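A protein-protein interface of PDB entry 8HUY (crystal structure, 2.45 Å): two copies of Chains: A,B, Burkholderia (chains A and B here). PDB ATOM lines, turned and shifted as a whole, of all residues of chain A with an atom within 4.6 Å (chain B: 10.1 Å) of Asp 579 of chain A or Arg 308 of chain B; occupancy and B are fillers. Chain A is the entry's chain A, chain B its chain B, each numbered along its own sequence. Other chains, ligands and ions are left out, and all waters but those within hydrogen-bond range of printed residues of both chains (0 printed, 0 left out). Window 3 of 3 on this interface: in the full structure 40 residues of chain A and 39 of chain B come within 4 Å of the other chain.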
ATOM      1  N   ARG A 313      27.754 -26.928 -22.256  1.00  0.00           N
ATOM      2  CA  ARG A 313      28.085 -27.933 -21.254  1.00  0.00           C
ATOM      3  C   ARG A 313      27.041 -29.023 -21.147  1.00  0.00           C
ATOM      4  O   ARG A 313      27.360 -30.091 -20.632  1.00  0.00           O
ATOM      5  CB  ARG A 313      28.255 -27.304 -19.871  1.00  0.00           C
ATOM      6  CG  ARG A 313      29.289 -26.200 -19.793  1.00  0.00           C
ATOM      7  CD  ARG A 313      29.397 -25.603 -18.355  1.00  0.00           C
ATOM      8  NE  ARG A 313      28.234 -25.834 -17.505  1.00  0.00           N
ATOM      9  CZ  ARG A 313      27.582 -24.874 -16.843  1.00  0.00           C
ATOM     10  NH1 ARG A 313      27.980 -23.604 -16.925  1.00  0.00           N
ATOM     11  NH2 ARG A 313      26.538 -25.188 -16.081  1.00  0.00           N
ATOM     12  N   VAL A 545      35.670 -12.237 -16.974  1.00  0.00           N
ATOM     13  CA  VAL A 545      36.562 -12.942 -17.883  1.00  0.00           C
ATOM     14  C   VAL A 545      36.632 -14.401 -17.465  1.00  0.00           C
ATOM     15  O   VAL A 545      36.437 -14.751 -16.298  1.00  0.00           O
ATOM     16  CB  VAL A 545      37.986 -12.336 -17.961  1.00  0.00           C
ATOM     17  CG1 VAL A 545      37.916 -10.847 -18.241  1.00  0.00           C
ATOM     18  CG2 VAL A 545      38.803 -12.651 -16.706  1.00  0.00           C
ATOM     19  N   GLY A 546      36.929 -15.253 -18.442  1.00  0.00           N
ATOM     20  CA  GLY A 546      37.135 -16.668 -18.219  1.00  0.00           C
ATOM     21  C   GLY A 546      38.599 -17.024 -18.403  1.00  0.00           C
ATOM     22  O   GLY A 546      39.328 -16.374 -19.154  1.00  0.00           O
ATOM     23  N   ARG A 547      39.026 -18.069 -17.716  1.00  0.00           N
ATOM     24  CA  ARG A 547      40.414 -18.486 -17.750  1.00  0.00           C
ATOM     25  C   ARG A 547      40.425 -19.932 -17.285  1.00  0.00           C
ATOM     26  O   ARG A 547      39.418 -20.449 -16.794  1.00  0.00           O
ATOM     27  CB  ARG A 547      41.289 -17.563 -16.896  1.00  0.00           C
ATOM     28  CG  ARG A 547      40.713 -17.344 -15.500  1.00  0.00           C
ATOM     29  CD  ARG A 547      41.798 -17.436 -14.419  1.00  0.00           C
ATOM     30  NE  ARG A 547      42.300 -18.796 -14.156  1.00  0.00           N
ATOM     31  CZ  ARG A 547      41.573 -19.802 -13.662  1.00  0.00           C
ATOM     32  NH1 ARG A 547      42.122 -20.993 -13.442  1.00  0.00           N
ATOM     33  NH2 ARG A 547      40.291 -19.629 -13.397  1.00  0.00           N
ATOM     34  N   HIS A 576      31.415 -19.252 -21.473  1.00  0.00           N
ATOM     35  CA  HIS A 576      32.838 -19.304 -21.816  1.00  0.00           C
ATOM     36  C   HIS A 576      33.266 -20.711 -22.230  1.00  0.00           C
ATOM     37  O   HIS A 576      32.844 -21.709 -21.637  1.00  0.00           O
ATOM     38  CB  HIS A 576      33.737 -18.877 -20.649  1.00  0.00           C
ATOM     39  CG  HIS A 576      33.544 -17.469 -20.202  1.00  0.00           C
ATOM     40  ND1 HIS A 576      33.595 -17.105 -18.871  1.00  0.00           N
ATOM     41  CD2 HIS A 576      33.294 -16.334 -20.897  1.00  0.00           C
ATOM     42  CE1 HIS A 576      33.377 -15.807 -18.762  1.00  0.00           C
ATOM     43  NE2 HIS A 576      33.187 -15.316 -19.976  1.00  0.00           N
ATOM     44  N   ALA A 577      34.165 -20.767 -23.217  1.00  0.00           N
ATOM     45  CA  ALA A 577      34.805 -22.023 -23.581  1.00  0.00           C
ATOM     46  C   ALA A 577      35.828 -22.458 -22.537  1.00  0.00           C
ATOM     47  O   ALA A 577      35.887 -23.641 -22.187  1.00  0.00           O
ATOM     48  CB  ALA A 577      35.487 -21.880 -24.941  1.00  0.00           C
ATOM     49  N   LEU A 578      36.626 -21.519 -22.008  1.00  0.00           N
ATOM     50  CA  LEU A 578      37.752 -21.911 -21.159  1.00  0.00           C
ATOM     51  C   LEU A 578      37.289 -22.474 -19.818  1.00  0.00           C
ATOM     52  O   LEU A 578      37.904 -23.416 -19.301  1.00  0.00           O
ATOM     53  CB  LEU A 578      38.688 -20.732 -20.927  1.00  0.00           C
ATOM     54  CG  LEU A 578      39.435 -20.161 -22.142  1.00  0.00           C
ATOM     55  CD1 LEU A 578      40.256 -18.962 -21.727  1.00  0.00           C
ATOM     56  CD2 LEU A 578      40.320 -21.203 -22.802  1.00  0.00           C
ATOM     57  N   ASP A 579      36.204 -21.922 -19.226  1.00  0.00           N
ATOM     58  CA  ASP A 579      35.799 -22.346 -17.886  1.00  0.00           C
ATOM     59  C   ASP A 579      34.327 -22.681 -17.722  1.00  0.00           C
ATOM     60  O   ASP A 579      33.932 -23.060 -16.624  1.00  0.00           O
ATOM     61  CB  ASP A 579      36.193 -21.293 -16.828  1.00  0.00           C
ATOM     62  CG  ASP A 579      35.529 -19.921 -17.028  1.00  0.00           C
ATOM     63  OD1 ASP A 579      36.096 -18.963 -16.486  1.00  0.00           O
ATOM     64  OD2 ASP A 579      34.456 -19.772 -17.662  1.00  0.00           O
ATOM     65  N   GLY A 580      33.531 -22.625 -18.785  1.00  0.00           N
ATOM     66  CA  GLY A 580      32.136 -22.993 -18.736  1.00  0.00           C
ATOM     67  C   GLY A 580      31.201 -22.008 -18.057  1.00  0.00           C
ATOM     68  O   GLY A 580      29.996 -22.272 -18.019  1.00  0.00           O
ATOM     69  N   GLU A 581      31.699 -20.882 -17.537  1.00  0.00           N
ATOM     70  CA  GLU A 581      30.856 -19.931 -16.825  1.00  0.00           C
ATOM     71  C   GLU A 581      30.120 -19.000 -17.788  1.00  0.00           C
ATOM     72  O   GLU A 581      30.541 -18.764 -18.924  1.00  0.00           O
ATOM     73  CB  GLU A 581      31.674 -19.075 -15.843  1.00  0.00           C
ATOM     74  CG  GLU A 581      32.637 -19.818 -14.911  1.00  0.00           C
ATOM     75  CD  GLU A 581      31.934 -20.541 -13.777  1.00  0.00           C
ATOM     76  OE1 GLU A 581      32.628 -21.109 -12.907  1.00  0.00           O
ATOM     77  OE2 GLU A 581      30.690 -20.551 -13.746  1.00  0.00           O
ATOM     78  N   ARG B 301      14.645 -18.332  -9.032  1.00  0.00           N
ATOM     79  CA  ARG B 301      15.780 -18.754  -8.235  1.00  0.00           C
ATOM     80  C   ARG B 301      15.349 -19.123  -6.822  1.00  0.00           C
ATOM     81  O   ARG B 301      14.497 -18.459  -6.221  1.00  0.00           O
ATOM     82  CB  ARG B 301      16.832 -17.642  -8.196  1.00  0.00           C
ATOM     83  CG  ARG B 301      17.463 -17.295  -9.558  1.00  0.00           C
ATOM     84  CD  ARG B 301      18.606 -16.271  -9.392  1.00  0.00           C
ATOM     85  NE  ARG B 301      18.139 -15.046  -8.749  1.00  0.00           N
ATOM     86  CZ  ARG B 301      18.647 -13.840  -8.993  1.00  0.00           C
ATOM     87  NH1 ARG B 301      19.638 -13.702  -9.873  1.00  0.00           N
ATOM     88  NH2 ARG B 301      18.151 -12.768  -8.383  1.00  0.00           N
ATOM     89  N   ALA B 304      19.543 -22.158  -3.108  1.00  0.00           N
ATOM     90  CA  ALA B 304      20.782 -22.815  -3.500  1.00  0.00           C
ATOM     91  C   ALA B 304      21.418 -22.205  -4.760  1.00  0.00           C
ATOM     92  O   ALA B 304      22.584 -22.502  -5.046  1.00  0.00           O
ATOM     93  CB  ALA B 304      20.527 -24.312  -3.704  1.00  0.00           C
ATOM     94  N   TRP B 305      20.689 -21.362  -5.497  1.00  0.00           N
ATOM     95  CA  TRP B 305      21.191 -20.777  -6.737  1.00  0.00           C
ATOM     96  C   TRP B 305      22.472 -20.008  -6.474  1.00  0.00           C
ATOM     97  O   TRP B 305      22.522 -19.170  -5.571  1.00  0.00           O
ATOM     98  CB  TRP B 305      20.142 -19.834  -7.332  1.00  0.00           C
ATOM     99  CG  TRP B 305      20.371 -19.403  -8.793  1.00  0.00           C
ATOM    100  CD1 TRP B 305      19.833 -19.980  -9.900  1.00  0.00           C
ATOM    101  CD2 TRP B 305      21.148 -18.274  -9.265  1.00  0.00           C
ATOM    102  NE1 TRP B 305      20.225 -19.295 -11.032  1.00  0.00           N
ATOM    103  CE2 TRP B 305      21.036 -18.249 -10.668  1.00  0.00           C
ATOM    104  CE3 TRP B 305      21.917 -17.284  -8.631  1.00  0.00           C
ATOM    105  CZ2 TRP B 305      21.669 -17.285 -11.456  1.00  0.00           C
ATOM    106  CZ3 TRP B 305      22.538 -16.322  -9.404  1.00  0.00           C
ATOM    107  CH2 TRP B 305      22.414 -16.332 -10.812  1.00  0.00           C
ATOM    108  N   ASN B 306      23.502 -20.289  -7.270  1.00  0.00           N
ATOM    109  CA  ASN B 306      24.808 -19.646  -7.123  1.00  0.00           C
ATOM    110  C   ASN B 306      25.349 -19.078  -8.425  1.00  0.00           C
ATOM    111  O   ASN B 306      26.494 -18.613  -8.443  1.00  0.00           O
ATOM    112  CB  ASN B 306      25.838 -20.635  -6.572  1.00  0.00           C
ATOM    113  CG  ASN B 306      25.977 -21.855  -7.461  1.00  0.00           C
ATOM    114  OD1 ASN B 306      25.776 -21.780  -8.684  1.00  0.00           O
ATOM    115  ND2 ASN B 306      26.301 -22.984  -6.861  1.00  0.00           N
ATOM    116  N   GLY B 307      24.617 -19.188  -9.530  1.00  0.00           N
ATOM    117  CA  GLY B 307      25.066 -18.608 -10.778  1.00  0.00           C
ATOM    118  C   GLY B 307      25.728 -19.580 -11.743  1.00  0.00           C
ATOM    119  O   GLY B 307      25.892 -19.234 -12.915  1.00  0.00           O
ATOM    120  N   ARG B 308      26.091 -20.786 -11.290  1.00  0.00           N
ATOM    121  CA  ARG B 308      26.647 -21.783 -12.189  1.00  0.00           C
ATOM    122  C   ARG B 308      25.592 -22.377 -13.115  1.00  0.00           C
ATOM    123  O   ARG B 308      25.943 -22.920 -14.168  1.00  0.00           O
ATOM    124  CB  ARG B 308      27.330 -22.886 -11.375  1.00  0.00           C
ATOM    125  CG  ARG B 308      27.877 -24.051 -12.196  1.00  0.00           C
ATOM    126  CD  ARG B 308      29.022 -23.632 -13.127  1.00  0.00           C
ATOM    127  NE  ARG B 308      29.642 -24.822 -13.705  1.00  0.00           N
ATOM    128  CZ  ARG B 308      30.601 -24.813 -14.637  1.00  0.00           C
ATOM    129  NH1 ARG B 308      31.064 -23.653 -15.104  1.00  0.00           N
ATOM    130  NH2 ARG B 308      31.100 -25.970 -15.100  1.00  0.00           N
ATOM    131  N   GLU B 309      24.315 -22.257 -12.772  1.00  0.00           N
ATOM    132  CA  GLU B 309      23.218 -22.763 -13.588  1.00  0.00           C
ATOM    133  C   GLU B 309      22.236 -21.641 -13.927  1.00  0.00           C
ATOM    134  O   GLU B 309      21.911 -20.794 -13.080  1.00  0.00           O
ATOM    135  CB  GLU B 309      22.497 -23.910 -12.866  1.00  0.00           C
ATOM    136  CG  GLU B 309      23.422 -24.977 -12.313  1.00  0.00           C
ATOM    137  CD  GLU B 309      23.948 -25.938 -13.388  1.00  0.00           C
ATOM    138  OE1 GLU B 309      24.832 -26.773 -13.057  1.00  0.00           O
ATOM    139  OE2 GLU B 309      23.481 -25.859 -14.555  1.00  0.00           O
ATOM    140  N   ARG B 310      21.774 -21.644 -15.176  1.00  0.00           N
ATOM    141  CA  ARG B 310      20.857 -20.633 -15.683  1.00  0.00           C
ATOM    142  C   ARG B 310      19.609 -21.233 -16.315  1.00  0.00           C
ATOM    143  O   ARG B 310      18.793 -20.486 -16.868  1.00  0.00           O
ATOM    144  CB  ARG B 310      21.555 -19.748 -16.726  1.00  0.00           C
ATOM    145  CG  ARG B 310      22.882 -19.175 -16.269  1.00  0.00           C
ATOM    146  CD  ARG B 310      22.697 -18.299 -15.033  1.00  0.00           C
ATOM    147  NE  ARG B 310      23.974 -17.927 -14.427  1.00  0.00           N
ATOM    148  CZ  ARG B 310      24.492 -16.707 -14.476  1.00  0.00           C
ATOM    149  NH1 ARG B 310      23.845 -15.746 -15.122  1.00  0.00           N
ATOM    150  NH2 ARG B 310      25.657 -16.451 -13.885  1.00  0.00           N
ATOM    151  N   CYS B 311      19.458 -22.557 -16.289  1.00  0.00           N
ATOM    152  CA  CYS B 311      18.358 -23.243 -16.954  1.00  0.00           C
ATOM    153  C   CYS B 311      17.680 -24.185 -15.977  1.00  0.00           C
ATOM    154  O   CYS B 311      18.302 -25.150 -15.520  1.00  0.00           O
ATOM    155  CB  CYS B 311      18.840 -24.028 -18.179  1.00  0.00           C
ATOM    156  SG  CYS B 311      17.426 -24.565 -19.197  1.00  0.00           S
ATOM    157  N   TRP B 312      16.409 -23.911 -15.655  1.00  0.00           N
ATOM    158  CA  TRP B 312      15.718 -24.767 -14.689  1.00  0.00           C
ATOM    159  C   TRP B 312      15.527 -26.187 -15.211  1.00  0.00           C
ATOM    160  O   TRP B 312      15.424 -27.128 -14.407  1.00  0.00           O
ATOM    161  CB  TRP B 312      14.378 -24.157 -14.282  1.00  0.00           C
ATOM    162  CG  TRP B 312      13.332 -24.110 -15.344  1.00  0.00           C
ATOM    163  CD1 TRP B 312      12.968 -23.013 -16.096  1.00  0.00           C
ATOM    164  CD2 TRP B 312      12.457 -25.177 -15.740  1.00  0.00           C
ATOM    165  NE1 TRP B 312      11.929 -23.347 -16.945  1.00  0.00           N
ATOM    166  CE2 TRP B 312      11.602 -24.666 -16.747  1.00  0.00           C
ATOM    167  CE3 TRP B 312      12.321 -26.517 -15.355  1.00  0.00           C
ATOM    168  CZ2 TRP B 312      10.644 -25.454 -17.383  1.00  0.00           C
ATOM    169  CZ3 TRP B 312      11.359 -27.304 -15.988  1.00  0.00           C
ATOM    170  CH2 TRP B 312      10.528 -26.766 -16.983  1.00  0.00           C
ATOM    171  N   THR B 314      17.619 -28.206 -16.495  1.00  0.00           N
ATOM    172  CA  THR B 314      18.738 -29.097 -16.184  1.00  0.00           C
ATOM    173  C   THR B 314      19.325 -28.887 -14.802  1.00  0.00           C
ATOM    174  O   THR B 314      20.303 -29.559 -14.466  1.00  0.00           O
ATOM    175  CB  THR B 314      19.881 -28.971 -17.215  1.00  0.00           C
ATOM    176  OG1 THR B 314      20.481 -27.663 -17.154  1.00  0.00           O
ATOM    177  CG2 THR B 314      19.370 -29.275 -18.626  1.00  0.00           C
ATOM    178  N   ALA B 315      18.780 -27.974 -13.998  1.00  0.00           N
ATOM    179  CA  ALA B 315      19.263 -27.734 -12.637  1.00  0.00           C
ATOM    180  C   ALA B 315      18.086 -27.390 -11.717  1.00  0.00           C
ATOM    181  O   ALA B 315      18.013 -26.303 -11.149  1.00  0.00           O
ATOM    182  CB  ALA B 315      20.327 -26.636 -12.647  1.00  0.00           C
ATOM    183  N   HIS B 318      18.314 -25.618  -8.157  1.00  0.00           N
ATOM    184  CA  HIS B 318      18.529 -24.177  -8.070  1.00  0.00           C
ATOM    185  C   HIS B 318      17.253 -23.367  -8.293  1.00  0.00           C
ATOM    186  O   HIS B 318      17.299 -22.135  -8.214  1.00  0.00           O
ATOM    187  CB  HIS B 318      19.615 -23.756  -9.060  1.00  0.00           C
ATOM    188  CG  HIS B 318      20.989 -24.139  -8.631  1.00  0.00           C
ATOM    189  ND1 HIS B 318      22.126 -23.539  -9.141  1.00  0.00           N
ATOM    190  CD2 HIS B 318      21.418 -25.061  -7.736  1.00  0.00           C
ATOM    191  CE1 HIS B 318      23.195 -24.075  -8.576  1.00  0.00           C
ATOM    192  NE2 HIS B 318      22.794 -25.006  -7.723  1.00  0.00           N
ATOM    193  N   TYR B 319      16.124 -24.025  -8.568  1.00  0.00           N
ATOM    194  CA  TYR B 319      14.872 -23.333  -8.840  1.00  0.00           C
ATOM    195  C   TYR B 319      13.713 -23.897  -8.006  1.00  0.00           C
ATOM    196  O   TYR B 319      12.550 -23.882  -8.443  1.00  0.00           O
ATOM    197  CB  TYR B 319      14.570 -23.394 -10.337  1.00  0.00           C
ATOM    198  CG  TYR B 319      15.614 -22.637 -11.150  1.00  0.00           C
ATOM    199  CD1 TYR B 319      16.859 -23.212 -11.449  1.00  0.00           C
ATOM    200  CD2 TYR B 319      15.376 -21.331 -11.580  1.00  0.00           C
ATOM    201  CE1 TYR B 319      17.815 -22.509 -12.161  1.00  0.00           C
ATOM    202  CE2 TYR B 319      16.327 -20.624 -12.296  1.00  0.00           C
ATOM    203  CZ  TYR B 319      17.541 -21.220 -12.592  1.00  0.00           C
ATOM    204  OH  TYR B 319      18.486 -20.518 -13.300  1.00  0.00           O
ATOM    205  N   ALA B 571      18.745 -12.099 -13.633  1.00  0.00           N
ATOM    206  CA  ALA B 571      19.706 -13.070 -14.137  1.00  0.00           C
ATOM    207  C   ALA B 571      19.329 -14.473 -13.689  1.00  0.00           C
ATOM    208  O   ALA B 571      18.967 -14.694 -12.525  1.00  0.00           O
ATOM    209  CB  ALA B 571      21.099 -12.722 -13.627  1.00  0.00           C
ATOM    210  N   GLY B 572      19.390 -15.417 -14.622  1.00  0.00           N
ATOM    211  CA  GLY B 572      19.119 -16.803 -14.311  1.00  0.00           C
ATOM    212  C   GLY B 572      17.662 -17.202 -14.344  1.00  0.00           C
ATOM    213  O   GLY B 572      17.365 -18.380 -14.098  1.00  0.00           O
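Printed residues of chain A that touch a printed residue of chain B: Arg 313, Asp 579, Gly 580 and Glu 581. Of the 16 printed residues of chain B, 2 touch a printed residue of chain A. Among the printed residues, 5 pairs touch across the chains.
The backbone carbonyl oxygen of Glu 309 of chain B sits at hydrogen-bond distance from the side-chain hydroxyl of Tyr 319 of chain B, at 3.4 Å. The side-chain amide oxygen (OD1) of Asn 306 of chain B is in hydrogen-bond range of the backbone NH (N) of Arg 308 of chain B. The backbone carbonyl oxygen (O) of Glu 309 of chain B is in hydrogen-bond range of the indole nitrogen (NE1) of Trp 305 of chain B (3.0 Å). The backbone NH (N) of Arg 547 of chain A lies within hydrogen-bond range of the side-chain carboxylate (OD1) of Asp 579 of chain A, at 3.3 Å. The backbone carbonyl oxygen of Gly 580 of chain A lies within hydrogen-bond range of the guanidinium group of Arg 313 of chain A (2.7 Å). OD2 of Asp 579 of chain A lies within hydrogen-bond range of N of Glu 581 of chain A (3.0 Å).
Printed residues of chain B within 4 Å of Arg 313 of chain A: Arg 308 and Glu 309. No residue of chain B comes within 4 Å of His 576 of chain A. No residue of chain B comes within 4 Å of Ala 577 of chain A. No residue of chain B comes within 4 Å of Leu 578 of chain A. Asp 579 of chain A touches just one residue of chain B: Arg 308 (3.3 Å). Of chain B, only Arg 308 (3.4 Å) comes within 4 Å of Gly 580 of chain A. Glu 581 of chain A touches just one residue of chain B: Arg 308. Arg 308 of chain B touches just these residues of chain A: Arg 313 (3.0 Å), Asp 579 (3.3 Å), Gly 580 (3.4 Å) and Glu 581 (3.4 Å). Of the printed residues of chain A, Glu 309 of chain B touches Arg 313 (3.5 Å). Thr 314 of chain B touches none of the printed residues of chain A. Tyr 319 of chain B touches none of the printed residues of chain A. The nearest residue of chain B that does not touch Asp 579 of chain A is Gly 307 of chain B (9.6 Å).
The side-chain carboxylate (OE2) of Glu 581 of chain A lies within salt-bridge range of the guanidinium group (NH1) of Arg 308 of chain B, at 3.4 Å. The backbone carbonyl oxygen of Asp 579 of chain A is in hydrogen-bond range of the guanidinium group of Arg 308 of chain B (3.3 Å). The guanidinium group of Arg 308 of chain B lies close to the backbone carbonyl oxygen of Gly 580 of chain A (3.4 Å). NH2 of Arg 313 of chain A is in hydrogen-bond range of O of Arg 308 of chain B, at 3.0 Å. NH2 of Arg 313 of chain A lies within salt-bridge range of OE2 of Glu 309 of chain B (3.5 Å).
No position is printed for both chains. Of the 5 pairs that touch across the chains among the printed residues, none has its exchanged pair printed and touching as well.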
